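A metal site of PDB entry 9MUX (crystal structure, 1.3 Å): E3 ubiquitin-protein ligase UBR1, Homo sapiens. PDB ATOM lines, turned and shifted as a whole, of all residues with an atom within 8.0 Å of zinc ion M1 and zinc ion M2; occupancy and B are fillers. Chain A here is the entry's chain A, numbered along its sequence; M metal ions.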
ATOM      1  N   GLN A   6      22.479  -1.639   6.508  1.00  0.00           N
ATOM      2  CA  GLN A   6      23.719  -0.988   6.922  1.00  0.00           C
ATOM      3  C   GLN A   6      24.456  -0.380   5.736  1.00  0.00           C
ATOM      4  O   GLN A   6      24.995   0.727   5.831  1.00  0.00           O
ATOM      5  CB  GLN A   6      24.606  -2.001   7.647  1.00  0.00           C
ATOM      6  CG  GLN A   6      24.960  -3.232   6.789  1.00  0.00           C
ATOM      7  CD  GLN A   6      25.743  -4.307   7.515  1.00  0.00           C
ATOM      8  OE1 GLN A   6      25.882  -4.282   8.735  1.00  0.00           O
ATOM      9  NE2 GLN A   6      26.279  -5.249   6.745  1.00  0.00           N
ATOM     10  N   LEU A   7      24.493  -1.089   4.623  1.00  0.00           N
ATOM     11  CA  LEU A   7      25.070  -0.611   3.385  1.00  0.00           C
ATOM     12  C   LEU A   7      23.932  -0.338   2.419  1.00  0.00           C
ATOM     13  O   LEU A   7      22.774  -0.701   2.663  1.00  0.00           O
ATOM     14  CB  LEU A   7      26.022  -1.670   2.805  1.00  0.00           C
ATOM     15  CG  LEU A   7      27.147  -2.017   3.789  1.00  0.00           C
ATOM     16  CD1 LEU A   7      27.680  -3.415   3.507  1.00  0.00           C
ATOM     17  CD2 LEU A   7      28.256  -0.967   3.741  1.00  0.00           C
ATOM     18  N   CYS A   8      24.264   0.313   1.323  1.00  0.00           N
ATOM     19  CA  CYS A   8      23.231   0.698   0.377  1.00  0.00           C
ATOM     20  C   CYS A   8      22.520  -0.512  -0.227  1.00  0.00           C
ATOM     21  O   CYS A   8      21.318  -0.720   0.010  1.00  0.00           O
ATOM     22  CB  CYS A   8      23.816   1.529  -0.757  1.00  0.00           C
ATOM     23  SG  CYS A   8      22.496   1.974  -1.883  1.00  0.00           S
ATOM     24  N   GLY A   9      23.241  -1.274  -1.036  1.00  0.00           N
ATOM     25  CA  GLY A   9      22.672  -2.435  -1.702  1.00  0.00           C
ATOM     26  C   GLY A   9      21.458  -2.164  -2.570  1.00  0.00           C
ATOM     27  O   GLY A   9      20.642  -3.076  -2.769  1.00  0.00           O
ATOM     28  N   ARG A  10      21.338  -0.979  -3.161  1.00  0.00           N
ATOM     29  CA  ARG A  10      20.168  -0.727  -4.004  1.00  0.00           C
ATOM     30  C   ARG A  10      20.244  -1.632  -5.230  1.00  0.00           C
ATOM     31  O   ARG A  10      21.276  -1.699  -5.904  1.00  0.00           O
ATOM     32  CB  ARG A  10      20.114   0.730  -4.437  1.00  0.00           C
ATOM     33  CG  ARG A  10      18.798   1.071  -5.144  1.00  0.00           C
ATOM     34  CD  ARG A  10      18.784   2.442  -5.777  1.00  0.00           C
ATOM     35  NE  ARG A  10      17.478   2.764  -6.327  1.00  0.00           N
ATOM     36  CZ  ARG A  10      16.567   3.515  -5.709  1.00  0.00           C
ATOM     37  NH1 ARG A  10      16.808   4.046  -4.525  1.00  0.00           N
ATOM     38  NH2 ARG A  10      15.402   3.734  -6.304  1.00  0.00           N
ATOM     39  N   VAL A  11      19.169  -2.360  -5.511  1.00  0.00           N
ATOM     40  CA  VAL A  11      19.059  -3.174  -6.728  1.00  0.00           C
ATOM     41  C   VAL A  11      18.313  -2.347  -7.760  1.00  0.00           C
ATOM     42  O   VAL A  11      17.183  -1.908  -7.518  1.00  0.00           O
ATOM     43  CB  VAL A  11      18.331  -4.503  -6.465  1.00  0.00           C
ATOM     44  CG1 VAL A  11      18.064  -5.227  -7.777  1.00  0.00           C
ATOM     45  CG2 VAL A  11      19.145  -5.376  -5.545  1.00  0.00           C
ATOM     46  N   PHE A  12      18.927  -2.131  -8.911  1.00  0.00           N
ATOM     47  CA  PHE A  12      18.345  -1.256  -9.917  1.00  0.00           C
ATOM     48  C   PHE A  12      17.183  -1.912 -10.644  1.00  0.00           C
ATOM     49  O   PHE A  12      17.213  -3.112 -10.922  1.00  0.00           O
ATOM     50  CB  PHE A  12      19.411  -0.829 -10.926  1.00  0.00           C
ATOM     51  CG  PHE A  12      20.504  -0.050 -10.292  1.00  0.00           C
ATOM     52  CD1 PHE A  12      20.259   1.214  -9.782  1.00  0.00           C
ATOM     53  CD2 PHE A  12      21.780  -0.587 -10.182  1.00  0.00           C
ATOM     54  CE1 PHE A  12      21.265   1.952  -9.178  1.00  0.00           C
ATOM     55  CE2 PHE A  12      22.800   0.147  -9.577  1.00  0.00           C
ATOM     56  CZ  PHE A  12      22.542   1.416  -9.068  1.00  0.00           C
ATOM     57  N   VAL A  31      29.445   0.575 -10.015  1.00  0.00           N
ATOM     58  CA  VAL A  31      28.401   1.570 -10.202  1.00  0.00           C
ATOM     59  C   VAL A  31      27.854   2.013  -8.851  1.00  0.00           C
ATOM     60  O   VAL A  31      27.991   1.328  -7.850  1.00  0.00           O
ATOM     61  CB  VAL A  31      27.234   1.039 -11.087  1.00  0.00           C
ATOM     62  CG1 VAL A  31      27.683   0.836 -12.529  1.00  0.00           C
ATOM     63  CG2 VAL A  31      26.654  -0.258 -10.486  1.00  0.00           C
ATOM     64  N   LEU A  32      27.221   3.175  -8.871  1.00  0.00           N
ATOM     65  CA  LEU A  32      26.583   3.742  -7.702  1.00  0.00           C
ATOM     66  C   LEU A  32      25.162   4.145  -8.063  1.00  0.00           C
ATOM     67  O   LEU A  32      24.894   4.574  -9.192  1.00  0.00           O
ATOM     68  CB  LEU A  32      27.322   4.992  -7.262  1.00  0.00           C
ATOM     69  CG  LEU A  32      28.753   4.797  -6.701  1.00  0.00           C
ATOM     70  CD1 LEU A  32      29.423   6.161  -6.492  1.00  0.00           C
ATOM     71  CD2 LEU A  32      28.767   3.998  -5.414  1.00  0.00           C
ATOM     72  N   CYS A  33      24.267   4.031  -7.092  1.00  0.00           N
ATOM     73  CA  CYS A  33      22.962   4.642  -7.268  1.00  0.00           C
ATOM     74  C   CYS A  33      23.098   6.163  -7.194  1.00  0.00           C
ATOM     75  O   CYS A  33      24.139   6.705  -6.820  1.00  0.00           O
ATOM     76  CB  CYS A  33      21.965   4.141  -6.209  1.00  0.00           C
ATOM     77  SG  CYS A  33      22.297   4.758  -4.515  1.00  0.00           S
ATOM     78  N   MET A  34      22.046   6.860  -7.621  1.00  0.00           N
ATOM     79  CA  MET A  34      22.092   8.306  -7.683  1.00  0.00           C
ATOM     80  C   MET A  34      22.370   8.922  -6.319  1.00  0.00           C
ATOM     81  O   MET A  34      23.177   9.854  -6.212  1.00  0.00           O
ATOM     82  CB  MET A  34      20.788   8.866  -8.253  1.00  0.00           C
ATOM     83  CG  MET A  34      20.823  10.374  -8.467  1.00  0.00           C
ATOM     84  SD  MET A  34      19.230  11.034  -8.946  1.00  0.00           S
ATOM     85  CE  MET A  34      18.292  10.721  -7.468  1.00  0.00           C
ATOM     86  N   ASP A  35      21.707   8.431  -5.274  1.00  0.00           N
ATOM     87  CA  ASP A  35      21.898   9.006  -3.940  1.00  0.00           C
ATOM     88  C   ASP A  35      23.330   8.836  -3.462  1.00  0.00           C
ATOM     89  O   ASP A  35      23.947   9.787  -2.975  1.00  0.00           O
ATOM     90  CB  ASP A  35      20.945   8.382  -2.927  1.00  0.00           C
ATOM     91  CG  ASP A  35      19.502   8.702  -3.201  1.00  0.00           C
ATOM     92  OD1 ASP A  35      19.221   9.774  -3.755  1.00  0.00           O
ATOM     93  OD2 ASP A  35      18.653   7.875  -2.833  1.00  0.00           O
ATOM     94  N   CYS A  36      23.876   7.622  -3.597  1.00  0.00           N
ATOM     95  CA  CYS A  36      25.252   7.413  -3.160  1.00  0.00           C
ATOM     96  C   CYS A  36      26.225   8.246  -3.993  1.00  0.00           C
ATOM     97  O   CYS A  36      27.166   8.824  -3.447  1.00  0.00           O
ATOM     98  CB  CYS A  36      25.614   5.933  -3.186  1.00  0.00           C
ATOM     99  SG  CYS A  36      24.687   4.984  -1.946  1.00  0.00           S
ATOM    100  N   PHE A  37      25.996   8.330  -5.298  1.00  0.00           N
ATOM    101  CA  PHE A  37      26.850   9.162  -6.146  1.00  0.00           C
ATOM    102  C   PHE A  37      26.840  10.606  -5.648  1.00  0.00           C
ATOM    103  O   PHE A  37      27.898  11.216  -5.456  1.00  0.00           O
ATOM    104  CB  PHE A  37      26.354   9.090  -7.591  1.00  0.00           C
ATOM    105  CG  PHE A  37      27.113   9.977  -8.516  1.00  0.00           C
ATOM    106  CD1 PHE A  37      28.399   9.651  -8.910  1.00  0.00           C
ATOM    107  CD2 PHE A  37      26.541  11.135  -9.010  1.00  0.00           C
ATOM    108  CE1 PHE A  37      29.109  10.471  -9.786  1.00  0.00           C
ATOM    109  CE2 PHE A  37      27.253  11.943  -9.880  1.00  0.00           C
ATOM    110  CZ  PHE A  37      28.527  11.607 -10.255  1.00  0.00           C
ATOM    111  N   ASP A  39      26.087  11.786  -2.828  1.00  0.00           N
ATOM    112  CA  ASP A  39      26.589  11.900  -1.463  1.00  0.00           C
ATOM    113  C   ASP A  39      28.039  11.498  -1.350  1.00  0.00           C
ATOM    114  O   ASP A  39      28.554  11.309  -0.230  1.00  0.00           O
ATOM    115  CB  ASP A  39      25.736  11.051  -0.516  1.00  0.00           C
ATOM    116  CG  ASP A  39      24.413  11.689  -0.188  1.00  0.00           C
ATOM    117  OD1 ASP A  39      24.301  12.934  -0.267  1.00  0.00           O
ATOM    118  OD2 ASP A  39      23.454  10.948   0.141  1.00  0.00           O
ATOM    119  N   SER A  40      28.729  11.353  -2.473  1.00  0.00           N
ATOM    120  CA  SER A  40      30.099  10.862  -2.496  1.00  0.00           C
ATOM    121  C   SER A  40      31.007  11.892  -3.169  1.00  0.00           C
ATOM    122  O   SER A  40      30.560  12.798  -3.865  1.00  0.00           O
ATOM    123  CB  SER A  40      30.210   9.536  -3.261  1.00  0.00           C
ATOM    124  OG  SER A  40      30.204   9.765  -4.663  1.00  0.00           O
ATOM    125  N   PHE A  57      23.524  -3.775  -8.933  1.00  0.00           N
ATOM    126  CA  PHE A  57      23.349  -3.238  -7.602  1.00  0.00           C
ATOM    127  C   PHE A  57      24.419  -2.200  -7.318  1.00  0.00           C
ATOM    128  O   PHE A  57      25.495  -2.208  -7.922  1.00  0.00           O
ATOM    129  CB  PHE A  57      23.334  -4.351  -6.545  1.00  0.00           C
ATOM    130  CG  PHE A  57      24.601  -5.165  -6.479  1.00  0.00           C
ATOM    131  CD1 PHE A  57      24.754  -6.287  -7.270  1.00  0.00           C
ATOM    132  CD2 PHE A  57      25.622  -4.819  -5.600  1.00  0.00           C
ATOM    133  CE1 PHE A  57      25.932  -7.052  -7.195  1.00  0.00           C
ATOM    134  CE2 PHE A  57      26.773  -5.575  -5.527  1.00  0.00           C
ATOM    135  CZ  PHE A  57      26.913  -6.692  -6.319  1.00  0.00           C
ATOM    136  N   CYS A  58      24.101  -1.289  -6.410  1.00  0.00           N
ATOM    137  CA  CYS A  58      25.005  -0.225  -6.015  1.00  0.00           C
ATOM    138  C   CYS A  58      26.223  -0.775  -5.268  1.00  0.00           C
ATOM    139  O   CYS A  58      26.099  -1.612  -4.370  1.00  0.00           O
ATOM    140  CB  CYS A  58      24.249   0.760  -5.125  1.00  0.00           C
ATOM    141  SG  CYS A  58      25.259   2.131  -4.548  1.00  0.00           S
ATOM    142  N   ASP A  59      27.405  -0.263  -5.626  1.00  0.00           N
ATOM    143  CA  ASP A  59      28.673  -0.686  -5.036  1.00  0.00           C
ATOM    144  C   ASP A  59      29.185   0.255  -3.967  1.00  0.00           C
ATOM    145  O   ASP A  59      30.370   0.188  -3.616  1.00  0.00           O
ATOM    146  CB  ASP A  59      29.725  -0.839  -6.121  1.00  0.00           C
ATOM    147  CG  ASP A  59      29.397  -1.956  -7.074  1.00  0.00           C
ATOM    148  OD1 ASP A  59      29.130  -3.091  -6.591  1.00  0.00           O
ATOM    149  OD2 ASP A  59      29.339  -1.729  -8.302  1.00  0.00           O
ATOM    150  N   CYS A  60      28.334   1.117  -3.428  1.00  0.00           N
ATOM    151  CA  CYS A  60      28.756   1.941  -2.314  1.00  0.00           C
ATOM    152  C   CYS A  60      29.286   1.053  -1.195  1.00  0.00           C
ATOM    153  O   CYS A  60      28.637   0.071  -0.806  1.00  0.00           O
ATOM    154  CB  CYS A  60      27.568   2.751  -1.817  1.00  0.00           C
ATOM    155  SG  CYS A  60      28.023   3.809  -0.388  1.00  0.00           S
ATOM    156  N   GLY A  61      30.487   1.366  -0.721  1.00  0.00           N
ATOM    157  CA  GLY A  61      31.051   0.667   0.412  1.00  0.00           C
ATOM    158  C   GLY A  61      32.049  -0.417   0.079  1.00  0.00           C
ATOM    159  O   GLY A  61      32.670  -0.959   0.995  1.00  0.00           O
ATOM    160  N   PRO A  70      35.364   4.948  -1.286  1.00  0.00           N
ATOM    161  CA  PRO A  70      34.392   3.881  -1.590  1.00  0.00           C
ATOM    162  C   PRO A  70      33.026   4.077  -0.964  1.00  0.00           C
ATOM    163  O   PRO A  70      32.068   3.464  -1.459  1.00  0.00           O
ATOM    164  CB  PRO A  70      35.067   2.625  -1.031  1.00  0.00           C
ATOM    165  CG  PRO A  70      35.949   3.141   0.053  1.00  0.00           C
ATOM    166  CD  PRO A  70      36.459   4.461  -0.418  1.00  0.00           C
ATOM    167  N   PHE A  71      32.889   4.872   0.090  1.00  0.00           N
ATOM    168  CA  PHE A  71      31.600   5.103   0.737  1.00  0.00           C
ATOM    169  C   PHE A  71      31.104   6.510   0.450  1.00  0.00           C
ATOM    170  O   PHE A  71      31.882   7.472   0.499  1.00  0.00           O
ATOM    171  CB  PHE A  71      31.719   4.995   2.276  1.00  0.00           C
ATOM    172  CG  PHE A  71      31.851   3.593   2.805  1.00  0.00           C
ATOM    173  CD1 PHE A  71      30.727   2.845   3.112  1.00  0.00           C
ATOM    174  CD2 PHE A  71      33.100   3.060   3.070  1.00  0.00           C
ATOM    175  CE1 PHE A  71      30.850   1.572   3.649  1.00  0.00           C
ATOM    176  CE2 PHE A  71      33.230   1.778   3.584  1.00  0.00           C
ATOM    177  CZ  PHE A  71      32.105   1.045   3.872  1.00  0.00           C
ATOM    178  N   CYS A  72      29.809   6.658   0.217  1.00  0.00           N
ATOM    179  CA  CYS A  72      29.192   7.964   0.325  1.00  0.00           C
ATOM    180  C   CYS A  72      29.101   8.363   1.801  1.00  0.00           C
ATOM    181  O   CYS A  72      29.278   7.553   2.705  1.00  0.00           O
ATOM    182  CB  CYS A  72      27.804   7.935  -0.324  1.00  0.00           C
ATOM    183  SG  CYS A  72      26.489   7.175   0.683  1.00  0.00           S
ATOM    184  N   VAL A  73      28.765   9.626   2.048  1.00  0.00           N
ATOM    185  CA  VAL A  73      28.827  10.098   3.423  1.00  0.00           C
ATOM    186  C   VAL A  73      27.803   9.391   4.309  1.00  0.00           C
ATOM    187  O   VAL A  73      28.069   9.124   5.494  1.00  0.00           O
ATOM    188  CB  VAL A  73      28.722  11.637   3.490  1.00  0.00           C
ATOM    189  CG1 VAL A  73      27.340  12.120   3.080  1.00  0.00           C
ATOM    190  CG2 VAL A  73      29.044  12.134   4.902  1.00  0.00           C
ATOM    191  N   ASN A  74      26.634   9.061   3.751  1.00  0.00           N
ATOM    192  CA  ASN A  74      25.574   8.418   4.518  1.00  0.00           C
ATOM    193  C   ASN A  74      26.017   7.037   5.003  1.00  0.00           C
ATOM    194  O   ASN A  74      25.757   6.672   6.152  1.00  0.00           O
ATOM    195  CB  ASN A  74      24.358   8.216   3.610  1.00  0.00           C
ATOM    196  CG  ASN A  74      23.479   9.444   3.489  1.00  0.00           C
ATOM    197  OD1 ASN A  74      22.393   9.371   2.895  1.00  0.00           O
ATOM    198  ND2 ASN A  74      23.928  10.572   4.020  1.00  0.00           N
ATOM    199  N   HIS A  75      26.654   6.257   4.144  1.00  0.00           N
ATOM    200  CA  HIS A  75      26.983   4.870   4.449  1.00  0.00           C
ATOM    201  C   HIS A  75      28.353   4.692   5.090  1.00  0.00           C
ATOM    202  O   HIS A  75      28.629   3.623   5.636  1.00  0.00           O
ATOM    203  CB  HIS A  75      26.847   3.996   3.199  1.00  0.00           C
ATOM    204  CG  HIS A  75      25.434   3.878   2.745  1.00  0.00           C
ATOM    205  ND1 HIS A  75      24.991   4.318   1.515  1.00  0.00           N
ATOM    206  CD2 HIS A  75      24.330   3.428   3.401  1.00  0.00           C
ATOM    207  CE1 HIS A  75      23.687   4.125   1.424  1.00  0.00           C
ATOM    208  NE2 HIS A  75      23.256   3.586   2.551  1.00  0.00           N
ATOM    209  N   GLU A  76      29.184   5.718   5.032  1.00  0.00           N
ATOM    210  CA  GLU A  76      30.512   5.634   5.587  1.00  0.00           C
ATOM    211  C   GLU A  76      30.441   5.289   7.065  1.00  0.00           C
ATOM    212  O   GLU A  76      29.726   5.966   7.806  1.00  0.00           O
ATOM    213  CB  GLU A  76      31.125   7.026   5.426  1.00  0.00           C
ATOM    214  CG  GLU A  76      32.604   7.113   5.684  1.00  0.00           C
ATOM    215  CD  GLU A  76      33.174   8.340   5.007  1.00  0.00           C
ATOM    216  OE1 GLU A  76      32.705   9.468   5.313  1.00  0.00           O
ATOM    217  OE2 GLU A  76      34.041   8.159   4.132  1.00  0.00           O
HETATM  218 ZN    ZN M   1      26.108   5.038  -0.061  1.00  0.00          ZN
HETATM  219 ZN    ZN M   2      23.683   3.306  -3.308  1.00  0.00          ZN
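SG of Cys 8 sits close to N of Arg 10. SG of Cys 72 lies close to N of Asn 74 (3.6 Å). The side-chain hydroxyl (OG) of Ser 40 sits close to the backbone carbonyl oxygen (O) of Cys 36 (3.4 Å). The backbone NH of Cys 60 sits close to the side-chain sulfur of Cys 58. N of Cys 58 lies within hydrogen-bond range of O of Arg 10 (2.9 Å). SG of Cys 33 lies close to N of Asp 35, at 3.8 Å.
Along chain A the residues within 4 Å of zinc ion M1 span positions 36 to 75.
Four residues have an atom within 4 Å of zinc ion M2: Cys 8, Cys 33, Cys 36 and Cys 58.
Zinc ion M1 is bound by ND1 of His 75 (2.1 Å), SG of Cys 72 (2.3 Å), SG of Cys 60 (2.3 Å) and SG of Cys 36 (2.4 Å). Zinc ion M1 has four donor atoms within binding distance.
Zinc ion M2 is bound by the side-chain sulfur (SG) of Cys 8 (2.3 Å), the side-chain sulfur (SG) of Cys 58 (2.3 Å), the side-chain sulfur (SG) of Cys 33 (2.3 Å) and the side-chain sulfur (SG) of Cys 36 (2.4 Å).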
